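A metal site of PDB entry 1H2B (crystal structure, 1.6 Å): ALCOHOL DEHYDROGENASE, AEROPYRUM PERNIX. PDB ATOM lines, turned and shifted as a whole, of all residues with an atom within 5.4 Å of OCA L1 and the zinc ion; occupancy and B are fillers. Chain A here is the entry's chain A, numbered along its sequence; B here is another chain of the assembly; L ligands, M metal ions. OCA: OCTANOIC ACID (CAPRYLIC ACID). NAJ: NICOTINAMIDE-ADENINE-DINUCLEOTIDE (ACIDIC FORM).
The guanidinium group of Arg 354 lies within salt-bridge range of an oxygen (O1N) of NAJ L2, 2.6 Å away.
OG1 of Thr 56 sits at hydrogen-bond distance from O2D of NAJ L2 (3.0 Å).
An oxygen (O7N) of NAJ L2 sits at hydrogen-bond distance from the backbone NH (N) of Val 309 (2.7 Å).
O2D of NAJ L2 lies within hydrogen-bond range of N of Thr 56 (3.5 Å).
The backbone NH (N) of Tyr 286 sits at hydrogen-bond distance from an oxygen (O3D) of NAJ L2 (3.2 Å).
The backbone carbonyl oxygen (O) of Tyr 286 is in hydrogen-bond range of an oxygen (O3D) of NAJ L2.
The side-chain hydroxyl (OG1) of Thr 56 lies close to an oxygen (O1) of OCA L1 (2.7 Å).
Residues that only touch the zinc ion: Thr 56.
Four residues have an atom within 4 Å of the zinc ion: Cys 54, Thr 56, His 79 and Asp 168.
Trp 65 touches OCA L1 (CH2 to C4, 3.9 Å).
Phe 128 touches OCA L1.
Leu 131 touches OCA L1 (CD2 to C4, 3.7 Å).
CD1 of Leu 308 touches C6 of OCA L1 (3.9 Å).
Val 309 touches OCA L1.
Arg 277 of chain B touches OCA L1.
Ser 299 of chain B touches OCA L1.
Hydrophobic or aromatic side chains that line OCA L1: Trp 65, His 79, Phe 128, Leu 131, Leu 308 and Val 309.
11 residues have an atom within 4 Å of OCA L1: Cys 54, Thr 56, Trp 65, His 79, Phe 128, Leu 131, Asp 168, Leu 308, Val 309, Arg 277 of chain B and Ser 299 of chain B.
The zinc ion is bound by an oxygen (O1) of OCA L1, 1.9 Å away.
The zinc ion is bound by NE2 of His 79 (2.0 Å).
OD1 of Asp 168 binds the zinc ion (2.1 Å).
The zinc ion is bound by SG of Cys 54, 2.3 Å away.
The backbone carbonyl oxygen of Ser 299 of chain B is in hydrogen-bond range of the guanidinium group of Arg 277 of chain B, 2.8 Å away.
The indole nitrogen (NE1) of Trp 65 sits at hydrogen-bond distance from the side-chain hydroxyl (OH) of Tyr 286 (2.9 Å).
The backbone carbonyl oxygen of Asp 168 is in hydrogen-bond range of the side-chain hydroxyl of Thr 172, at 2.7 Å.
NH2 of Arg 277 of chain B lies within hydrogen-bond range of O of Met 121 (3.1 Å).
The side-chain hydroxyl of Tyr 286 sits at hydrogen-bond distance from the side-chain hydroxyl of Thr 56 (2.8 Å).
The side-chain sulfur of Cys 54 lies close to the guanidinium group of Arg 354 (3.3 Å).
SG of Cys 54 sits close to N of Thr 56, 3.4 Å away.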
ATOM      1  N   CYS A  54      -2.004  -0.157 -31.451  1.00  0.00           N
ATOM      2  CA  CYS A  54      -2.508  -0.493 -30.136  1.00  0.00           C
ATOM      3  C   CYS A  54      -2.454   0.722 -29.202  1.00  0.00           C
ATOM      4  O   CYS A  54      -1.611   1.592 -29.380  1.00  0.00           O
ATOM      5  CB  CYS A  54      -1.619  -1.612 -29.560  1.00  0.00           C
ATOM      6  SG  CYS A  54      -2.091  -2.262 -27.948  1.00  0.00           S
ATOM      7  N   THR A  56      -1.163   0.651 -26.487  1.00  0.00           N
ATOM      8  CA  THR A  56       0.201   0.545 -25.940  1.00  0.00           C
ATOM      9  C   THR A  56       1.158   1.433 -26.709  1.00  0.00           C
ATOM     10  O   THR A  56       2.140   1.930 -26.119  1.00  0.00           O
ATOM     11  CB  THR A  56       0.644  -0.924 -25.967  1.00  0.00           C
ATOM     12  OG1 THR A  56      -0.017  -1.600 -24.891  1.00  0.00           O
ATOM     13  CG2 THR A  56       2.164  -1.088 -25.709  1.00  0.00           C
ATOM     14  N   TRP A  65       6.991   3.065 -20.805  1.00  0.00           N
ATOM     15  CA  TRP A  65       7.763   1.831 -20.753  1.00  0.00           C
ATOM     16  C   TRP A  65       9.283   2.065 -20.654  1.00  0.00           C
ATOM     17  O   TRP A  65      10.052   1.100 -20.624  1.00  0.00           O
ATOM     18  CB  TRP A  65       7.481   0.976 -21.986  1.00  0.00           C
ATOM     19  CG  TRP A  65       6.136   0.314 -21.895  1.00  0.00           C
ATOM     20  CD1 TRP A  65       4.958   0.728 -22.505  1.00  0.00           C
ATOM     21  CD2 TRP A  65       5.814  -0.856 -21.169  1.00  0.00           C
ATOM     22  NE1 TRP A  65       3.936  -0.142 -22.201  1.00  0.00           N
ATOM     23  CE2 TRP A  65       4.423  -1.119 -21.368  1.00  0.00           C
ATOM     24  CE3 TRP A  65       6.548  -1.746 -20.358  1.00  0.00           C
ATOM     25  CZ2 TRP A  65       3.774  -2.219 -20.805  1.00  0.00           C
ATOM     26  CZ3 TRP A  65       5.880  -2.842 -19.797  1.00  0.00           C
ATOM     27  CH2 TRP A  65       4.514  -3.051 -20.021  1.00  0.00           C
ATOM     28  N   HIS A  79       3.397  -4.028 -32.983  1.00  0.00           N
ATOM     29  CA  HIS A  79       3.544  -5.400 -32.412  1.00  0.00           C
ATOM     30  C   HIS A  79       2.336  -6.311 -32.710  1.00  0.00           C
ATOM     31  O   HIS A  79       2.149  -7.362 -32.048  1.00  0.00           O
ATOM     32  CB  HIS A  79       3.804  -5.319 -30.894  1.00  0.00           C
ATOM     33  CG  HIS A  79       2.778  -4.536 -30.126  1.00  0.00           C
ATOM     34  ND1 HIS A  79       2.835  -3.166 -29.987  1.00  0.00           N
ATOM     35  CD2 HIS A  79       1.667  -4.940 -29.458  1.00  0.00           C
ATOM     36  CE1 HIS A  79       1.799  -2.756 -29.275  1.00  0.00           C
ATOM     37  NE2 HIS A  79       1.071  -3.808 -28.922  1.00  0.00           N
ATOM     38  N   GLU A  80       1.553  -5.899 -33.702  1.00  0.00           N
ATOM     39  CA  GLU A  80       0.303  -6.600 -34.051  1.00  0.00           C
ATOM     40  C   GLU A  80       0.259  -6.908 -35.533  1.00  0.00           C
ATOM     41  O   GLU A  80      -0.393  -6.211 -36.344  1.00  0.00           O
ATOM     42  CB  GLU A  80      -0.867  -5.692 -33.662  1.00  0.00           C
ATOM     43  CG  GLU A  80      -2.225  -6.401 -33.626  1.00  0.00           C
ATOM     44  CD  GLU A  80      -3.241  -5.538 -32.889  1.00  0.00           C
ATOM     45  OE1 GLU A  80      -3.868  -4.694 -33.558  1.00  0.00           O
ATOM     46  OE2 GLU A  80      -3.431  -5.700 -31.659  1.00  0.00           O
ATOM     47  N   MET A 121       4.977 -15.649 -22.562  1.00  0.00           N
ATOM     48  CA  MET A 121       5.218 -14.288 -22.072  1.00  0.00           C
ATOM     49  C   MET A 121       6.052 -14.279 -20.839  1.00  0.00           C
ATOM     50  O   MET A 121       6.415 -13.207 -20.334  1.00  0.00           O
ATOM     51  CB  MET A 121       3.876 -13.565 -21.786  1.00  0.00           C
ATOM     52  CG  MET A 121       2.992 -13.427 -23.025  1.00  0.00           C
ATOM     53  SD  MET A 121       3.801 -12.519 -24.333  1.00  0.00           S
ATOM     54  CE  MET A 121       4.253 -10.933 -23.486  1.00  0.00           C
ATOM     55  N   LEU A 126      12.931 -13.016 -23.248  1.00  0.00           N
ATOM     56  CA  LEU A 126      11.899 -12.451 -24.132  1.00  0.00           C
ATOM     57  C   LEU A 126      12.358 -11.186 -24.875  1.00  0.00           C
ATOM     58  O   LEU A 126      12.877 -10.235 -24.257  1.00  0.00           O
ATOM     59  CB  LEU A 126      10.629 -12.163 -23.310  1.00  0.00           C
ATOM     60  CG  LEU A 126       9.420 -11.916 -24.224  1.00  0.00           C
ATOM     61  CD1 LEU A 126       8.254 -12.755 -23.780  1.00  0.00           C
ATOM     62  CD2 LEU A 126       9.060 -10.434 -24.264  1.00  0.00           C
ATOM     63  N   PHE A 128      10.423  -8.436 -27.880  1.00  0.00           N
ATOM     64  CA  PHE A 128       9.065  -8.119 -28.272  1.00  0.00           C
ATOM     65  C   PHE A 128       9.100  -7.069 -29.386  1.00  0.00           C
ATOM     66  O   PHE A 128       9.164  -5.868 -29.088  1.00  0.00           O
ATOM     67  CB  PHE A 128       8.363  -7.620 -27.006  1.00  0.00           C
ATOM     68  CG  PHE A 128       6.848  -7.739 -27.026  1.00  0.00           C
ATOM     69  CD1 PHE A 128       6.195  -8.709 -26.277  1.00  0.00           C
ATOM     70  CD2 PHE A 128       6.062  -6.859 -27.765  1.00  0.00           C
ATOM     71  CE1 PHE A 128       4.771  -8.820 -26.270  1.00  0.00           C
ATOM     72  CE2 PHE A 128       4.653  -6.944 -27.749  1.00  0.00           C
ATOM     73  CZ  PHE A 128       4.009  -7.915 -26.999  1.00  0.00           C
ATOM     74  N   LEU A 131       7.992  -3.241 -29.175  1.00  0.00           N
ATOM     75  CA  LEU A 131       7.991  -2.764 -27.787  1.00  0.00           C
ATOM     76  C   LEU A 131       9.362  -2.352 -27.338  1.00  0.00           C
ATOM     77  O   LEU A 131       9.516  -1.229 -26.886  1.00  0.00           O
ATOM     78  CB  LEU A 131       7.401  -3.778 -26.788  1.00  0.00           C
ATOM     79  CG  LEU A 131       6.072  -3.143 -26.333  1.00  0.00           C
ATOM     80  CD1 LEU A 131       4.879  -3.603 -27.158  1.00  0.00           C
ATOM     81  CD2 LEU A 131       5.810  -3.219 -24.855  1.00  0.00           C
ATOM     82  N   ASP A 168      -2.447  -9.349 -31.100  1.00  0.00           N
ATOM     83  CA  ASP A 168      -2.188  -8.723 -29.820  1.00  0.00           C
ATOM     84  C   ASP A 168      -3.491  -8.365 -29.123  1.00  0.00           C
ATOM     85  O   ASP A 168      -3.775  -8.860 -28.037  1.00  0.00           O
ATOM     86  CB  ASP A 168      -1.265  -7.493 -30.027  1.00  0.00           C
ATOM     87  CG  ASP A 168      -0.892  -6.858 -28.737  1.00  0.00           C
ATOM     88  OD1 ASP A 168      -1.354  -5.740 -28.483  1.00  0.00           O
ATOM     89  OD2 ASP A 168      -0.188  -7.430 -27.878  1.00  0.00           O
ATOM     90  N   THR A 172      -4.808 -11.112 -26.369  1.00  0.00           N
ATOM     91  CA  THR A 172      -4.890 -10.586 -24.993  1.00  0.00           C
ATOM     92  C   THR A 172      -6.315 -10.699 -24.456  1.00  0.00           C
ATOM     93  O   THR A 172      -6.527 -11.175 -23.333  1.00  0.00           O
ATOM     94  CB  THR A 172      -4.454  -9.134 -24.949  1.00  0.00           C
ATOM     95  OG1 THR A 172      -3.117  -9.055 -25.415  1.00  0.00           O
ATOM     96  CG2 THR A 172      -4.442  -8.618 -23.517  1.00  0.00           C
ATOM     97  N   TYR A 286      -3.655  -0.791 -18.678  1.00  0.00           N
ATOM     98  CA  TYR A 286      -2.783  -0.304 -17.609  1.00  0.00           C
ATOM     99  C   TYR A 286      -2.508   1.169 -17.815  1.00  0.00           C
ATOM    100  O   TYR A 286      -2.810   1.751 -18.833  1.00  0.00           O
ATOM    101  CB  TYR A 286      -1.478  -1.125 -17.581  1.00  0.00           C
ATOM    102  CG  TYR A 286      -0.736  -1.022 -18.889  1.00  0.00           C
ATOM    103  CD1 TYR A 286       0.194  -0.017 -19.125  1.00  0.00           C
ATOM    104  CD2 TYR A 286      -0.992  -1.934 -19.922  1.00  0.00           C
ATOM    105  CE1 TYR A 286       0.844   0.082 -20.356  1.00  0.00           C
ATOM    106  CE2 TYR A 286      -0.352  -1.840 -21.166  1.00  0.00           C
ATOM    107  CZ  TYR A 286       0.559  -0.808 -21.369  1.00  0.00           C
ATOM    108  OH  TYR A 286       1.152  -0.665 -22.568  1.00  0.00           O
ATOM    109  N   LEU A 308      -1.690 -10.941 -19.259  1.00  0.00           N
ATOM    110  CA  LEU A 308      -0.639 -10.436 -20.111  1.00  0.00           C
ATOM    111  C   LEU A 308      -0.621 -11.148 -21.458  1.00  0.00           C
ATOM    112  O   LEU A 308      -0.267 -12.344 -21.540  1.00  0.00           O
ATOM    113  CB  LEU A 308       0.712 -10.598 -19.383  1.00  0.00           C
ATOM    114  CG  LEU A 308       1.964 -10.243 -20.204  1.00  0.00           C
ATOM    115  CD1 LEU A 308       2.002  -8.739 -20.526  1.00  0.00           C
ATOM    116  CD2 LEU A 308       3.248 -10.668 -19.464  1.00  0.00           C
ATOM    117  N   VAL A 309      -0.988 -10.407 -22.513  1.00  0.00           N
ATOM    118  CA  VAL A 309      -0.960 -10.937 -23.878  1.00  0.00           C
ATOM    119  C   VAL A 309      -1.500 -12.365 -23.861  1.00  0.00           C
ATOM    120  O   VAL A 309      -2.612 -12.584 -23.380  1.00  0.00           O
ATOM    121  CB  VAL A 309       0.417 -10.716 -24.595  1.00  0.00           C
ATOM    122  CG1 VAL A 309       0.295 -10.873 -26.118  1.00  0.00           C
ATOM    123  CG2 VAL A 309       0.974  -9.279 -24.295  1.00  0.00           C
ATOM    124  N   ARG A 354     -10.453  -1.355 -34.114  1.00  0.00           N
ATOM    125  CA  ARG A 354      -8.992  -1.384 -34.251  1.00  0.00           C
ATOM    126  C   ARG A 354      -8.518  -0.793 -35.554  1.00  0.00           C
ATOM    127  O   ARG A 354      -8.929  -1.224 -36.595  1.00  0.00           O
ATOM    128  CB  ARG A 354      -8.506  -2.842 -34.185  1.00  0.00           C
ATOM    129  CG  ARG A 354      -7.016  -3.059 -33.945  1.00  0.00           C
ATOM    130  CD  ARG A 354      -6.458  -2.299 -32.782  1.00  0.00           C
ATOM    131  NE  ARG A 354      -5.478  -3.039 -32.030  1.00  0.00           N
ATOM    132  CZ  ARG A 354      -5.219  -2.758 -30.757  1.00  0.00           C
ATOM    133  NH1 ARG A 354      -5.893  -1.796 -30.117  1.00  0.00           N
ATOM    134  NH2 ARG A 354      -4.271  -3.478 -30.142  1.00  0.00           N
ATOM    135  N   ARG B 277       7.162 -13.545 -11.397  1.00  0.00           N
ATOM    136  CA  ARG B 277       6.263 -13.582 -12.564  1.00  0.00           C
ATOM    137  C   ARG B 277       5.184 -14.591 -12.291  1.00  0.00           C
ATOM    138  O   ARG B 277       5.430 -15.737 -11.808  1.00  0.00           O
ATOM    139  CB  ARG B 277       7.025 -13.945 -13.831  1.00  0.00           C
ATOM    140  CG  ARG B 277       8.046 -12.885 -14.217  1.00  0.00           C
ATOM    141  CD  ARG B 277       8.650 -13.055 -15.632  1.00  0.00           C
ATOM    142  NE  ARG B 277       7.707 -12.644 -16.671  1.00  0.00           N
ATOM    143  CZ  ARG B 277       7.371 -11.384 -16.967  1.00  0.00           C
ATOM    144  NH1 ARG B 277       7.912 -10.331 -16.352  1.00  0.00           N
ATOM    145  NH2 ARG B 277       6.481 -11.169 -17.939  1.00  0.00           N
ATOM    146  N   ILE B 298       0.162  -6.041 -14.918  1.00  0.00           N
ATOM    147  CA  ILE B 298       0.137  -6.773 -16.193  1.00  0.00           C
ATOM    148  C   ILE B 298       1.537  -7.243 -16.609  1.00  0.00           C
ATOM    149  O   ILE B 298       1.667  -8.372 -17.118  1.00  0.00           O
ATOM    150  CB  ILE B 298      -0.647  -5.994 -17.308  1.00  0.00           C
ATOM    151  CG1 ILE B 298       0.141  -4.802 -17.838  1.00  0.00           C
ATOM    152  CG2 ILE B 298      -2.017  -5.566 -16.793  1.00  0.00           C
ATOM    153  CD1 ILE B 298       1.034  -5.092 -19.035  1.00  0.00           C
ATOM    154  N   SER B 299       2.587  -6.447 -16.406  1.00  0.00           N
ATOM    155  CA  SER B 299       3.890  -6.873 -16.963  1.00  0.00           C
ATOM    156  C   SER B 299       4.451  -8.098 -16.237  1.00  0.00           C
ATOM    157  O   SER B 299       5.163  -8.880 -16.871  1.00  0.00           O
ATOM    158  CB  SER B 299       4.903  -5.733 -17.050  1.00  0.00           C
ATOM    159  OG  SER B 299       5.129  -5.260 -15.760  1.00  0.00           O
HETATM  160  C1  OCA L   1       0.917  -5.026 -25.517  1.00  0.00           C
HETATM  161  C2  OCA L   1       1.597  -4.850 -24.167  1.00  0.00           C
HETATM  162  C3  OCA L   1       2.647  -5.946 -23.954  1.00  0.00           C
HETATM  163  C4  OCA L   1       3.706  -5.568 -22.920  1.00  0.00           C
HETATM  164  C5  OCA L   1       4.618  -6.776 -22.704  1.00  0.00           C
HETATM  165  C6  OCA L   1       5.264  -6.749 -21.322  1.00  0.00           C
HETATM  166  C7  OCA L   1       6.352  -7.837 -21.246  1.00  0.00           C
HETATM  167  C8  OCA L   1       6.590  -8.355 -19.829  1.00  0.00           C
HETATM  168  O1  OCA L   1       0.231  -4.054 -25.989  1.00  0.00           O
HETATM  169  O2  OCA L   1       1.108  -6.087 -26.166  1.00  0.00           O
HETATM  170  PA  NAJ L   2      -8.438   1.563 -27.032  1.00  0.00           P
HETATM  171  O1A NAJ L   2      -7.973   3.016 -26.972  1.00  0.00           O
HETATM  172  O2A NAJ L   2      -8.798   0.998 -28.397  1.00  0.00           O
HETATM  173  O5B NAJ L   2      -9.731   1.330 -26.168  1.00  0.00           O
HETATM  174  C5B NAJ L   2      -9.951   1.928 -24.891  1.00  0.00           C
HETATM  175  C4B NAJ L   2     -11.466   1.958 -24.721  1.00  0.00           C
HETATM  176  O4B NAJ L   2     -11.742   2.447 -23.427  1.00  0.00           O
HETATM  177  C3B NAJ L   2     -12.181   2.950 -25.693  1.00  0.00           C
HETATM  178  O3B NAJ L   2     -13.235   2.302 -26.382  1.00  0.00           O
HETATM  179  C2B NAJ L   2     -12.562   4.091 -24.775  1.00  0.00           C
HETATM  180  O2B NAJ L   2     -13.645   4.905 -25.215  1.00  0.00           O
HETATM  181  C1B NAJ L   2     -12.851   3.345 -23.488  1.00  0.00           C
HETATM  182  N9A NAJ L   2     -12.817   4.208 -22.316  1.00  0.00           N
HETATM  183  C8A NAJ L   2     -12.048   5.320 -22.045  1.00  0.00           C
HETATM  184  N7A NAJ L   2     -12.352   5.743 -20.802  1.00  0.00           N
HETATM  185  C5A NAJ L   2     -13.310   4.917 -20.269  1.00  0.00           C
HETATM  186  C6A NAJ L   2     -14.011   4.898 -19.070  1.00  0.00           C
HETATM  187  N6A NAJ L   2     -13.820   5.807 -18.100  1.00  0.00           N
HETATM  188  N1A NAJ L   2     -14.933   3.888 -18.823  1.00  0.00           N
HETATM  189  C2A NAJ L   2     -15.184   2.961 -19.838  1.00  0.00           C
HETATM  190  N3A NAJ L   2     -14.527   2.981 -21.013  1.00  0.00           N
HETATM  191  C4A NAJ L   2     -13.596   3.951 -21.236  1.00  0.00           C
HETATM  192  O3  NAJ L   2      -7.267   0.735 -26.320  1.00  0.00           O
HETATM  193  PN  NAJ L   2      -6.791  -0.776 -26.611  1.00  0.00           P
HETATM  194  O1N NAJ L   2      -5.784  -0.751 -27.685  1.00  0.00           O
HETATM  195  O2N NAJ L   2      -7.995  -1.627 -26.655  1.00  0.00           O
HETATM  196  O5D NAJ L   2      -6.011  -1.043 -25.243  1.00  0.00           O
HETATM  197  C5D NAJ L   2      -6.746  -1.121 -24.032  1.00  0.00           C
HETATM  198  C4D NAJ L   2      -5.811  -1.128 -22.806  1.00  0.00           C
HETATM  199  O4D NAJ L   2      -5.115  -2.400 -22.797  1.00  0.00           O
HETATM  200  C3D NAJ L   2      -4.667  -0.101 -22.909  1.00  0.00           C
HETATM  201  O3D NAJ L   2      -4.341   0.317 -21.603  1.00  0.00           O
HETATM  202  C2D NAJ L   2      -3.528  -0.864 -23.550  1.00  0.00           C
HETATM  203  O2D NAJ L   2      -2.259  -0.297 -23.343  1.00  0.00           O
HETATM  204  C1D NAJ L   2      -3.709  -2.180 -22.803  1.00  0.00           C
HETATM  205  N1N NAJ L   2      -3.030  -3.365 -23.358  1.00  0.00           N
HETATM  206  C2N NAJ L   2      -2.793  -4.367 -22.458  1.00  0.00           C
HETATM  207  C3N NAJ L   2      -2.262  -5.563 -22.906  1.00  0.00           C
HETATM  208  C7N NAJ L   2      -1.939  -6.623 -21.880  1.00  0.00           C
HETATM  209  O7N NAJ L   2      -1.338  -7.698 -22.361  1.00  0.00           O
HETATM  210  N7N NAJ L   2      -2.226  -6.487 -20.597  1.00  0.00           N
HETATM  211  C4N NAJ L   2      -2.021  -5.823 -24.288  1.00  0.00           C
HETATM  212  C5N NAJ L   2      -2.442  -4.824 -25.209  1.00  0.00           C
HETATM  213  C6N NAJ L   2      -2.957  -3.631 -24.718  1.00  0.00           C
HETATM  214 ZN    ZN M   1      -0.570  -3.911 -27.753  1.00  0.00          ZN
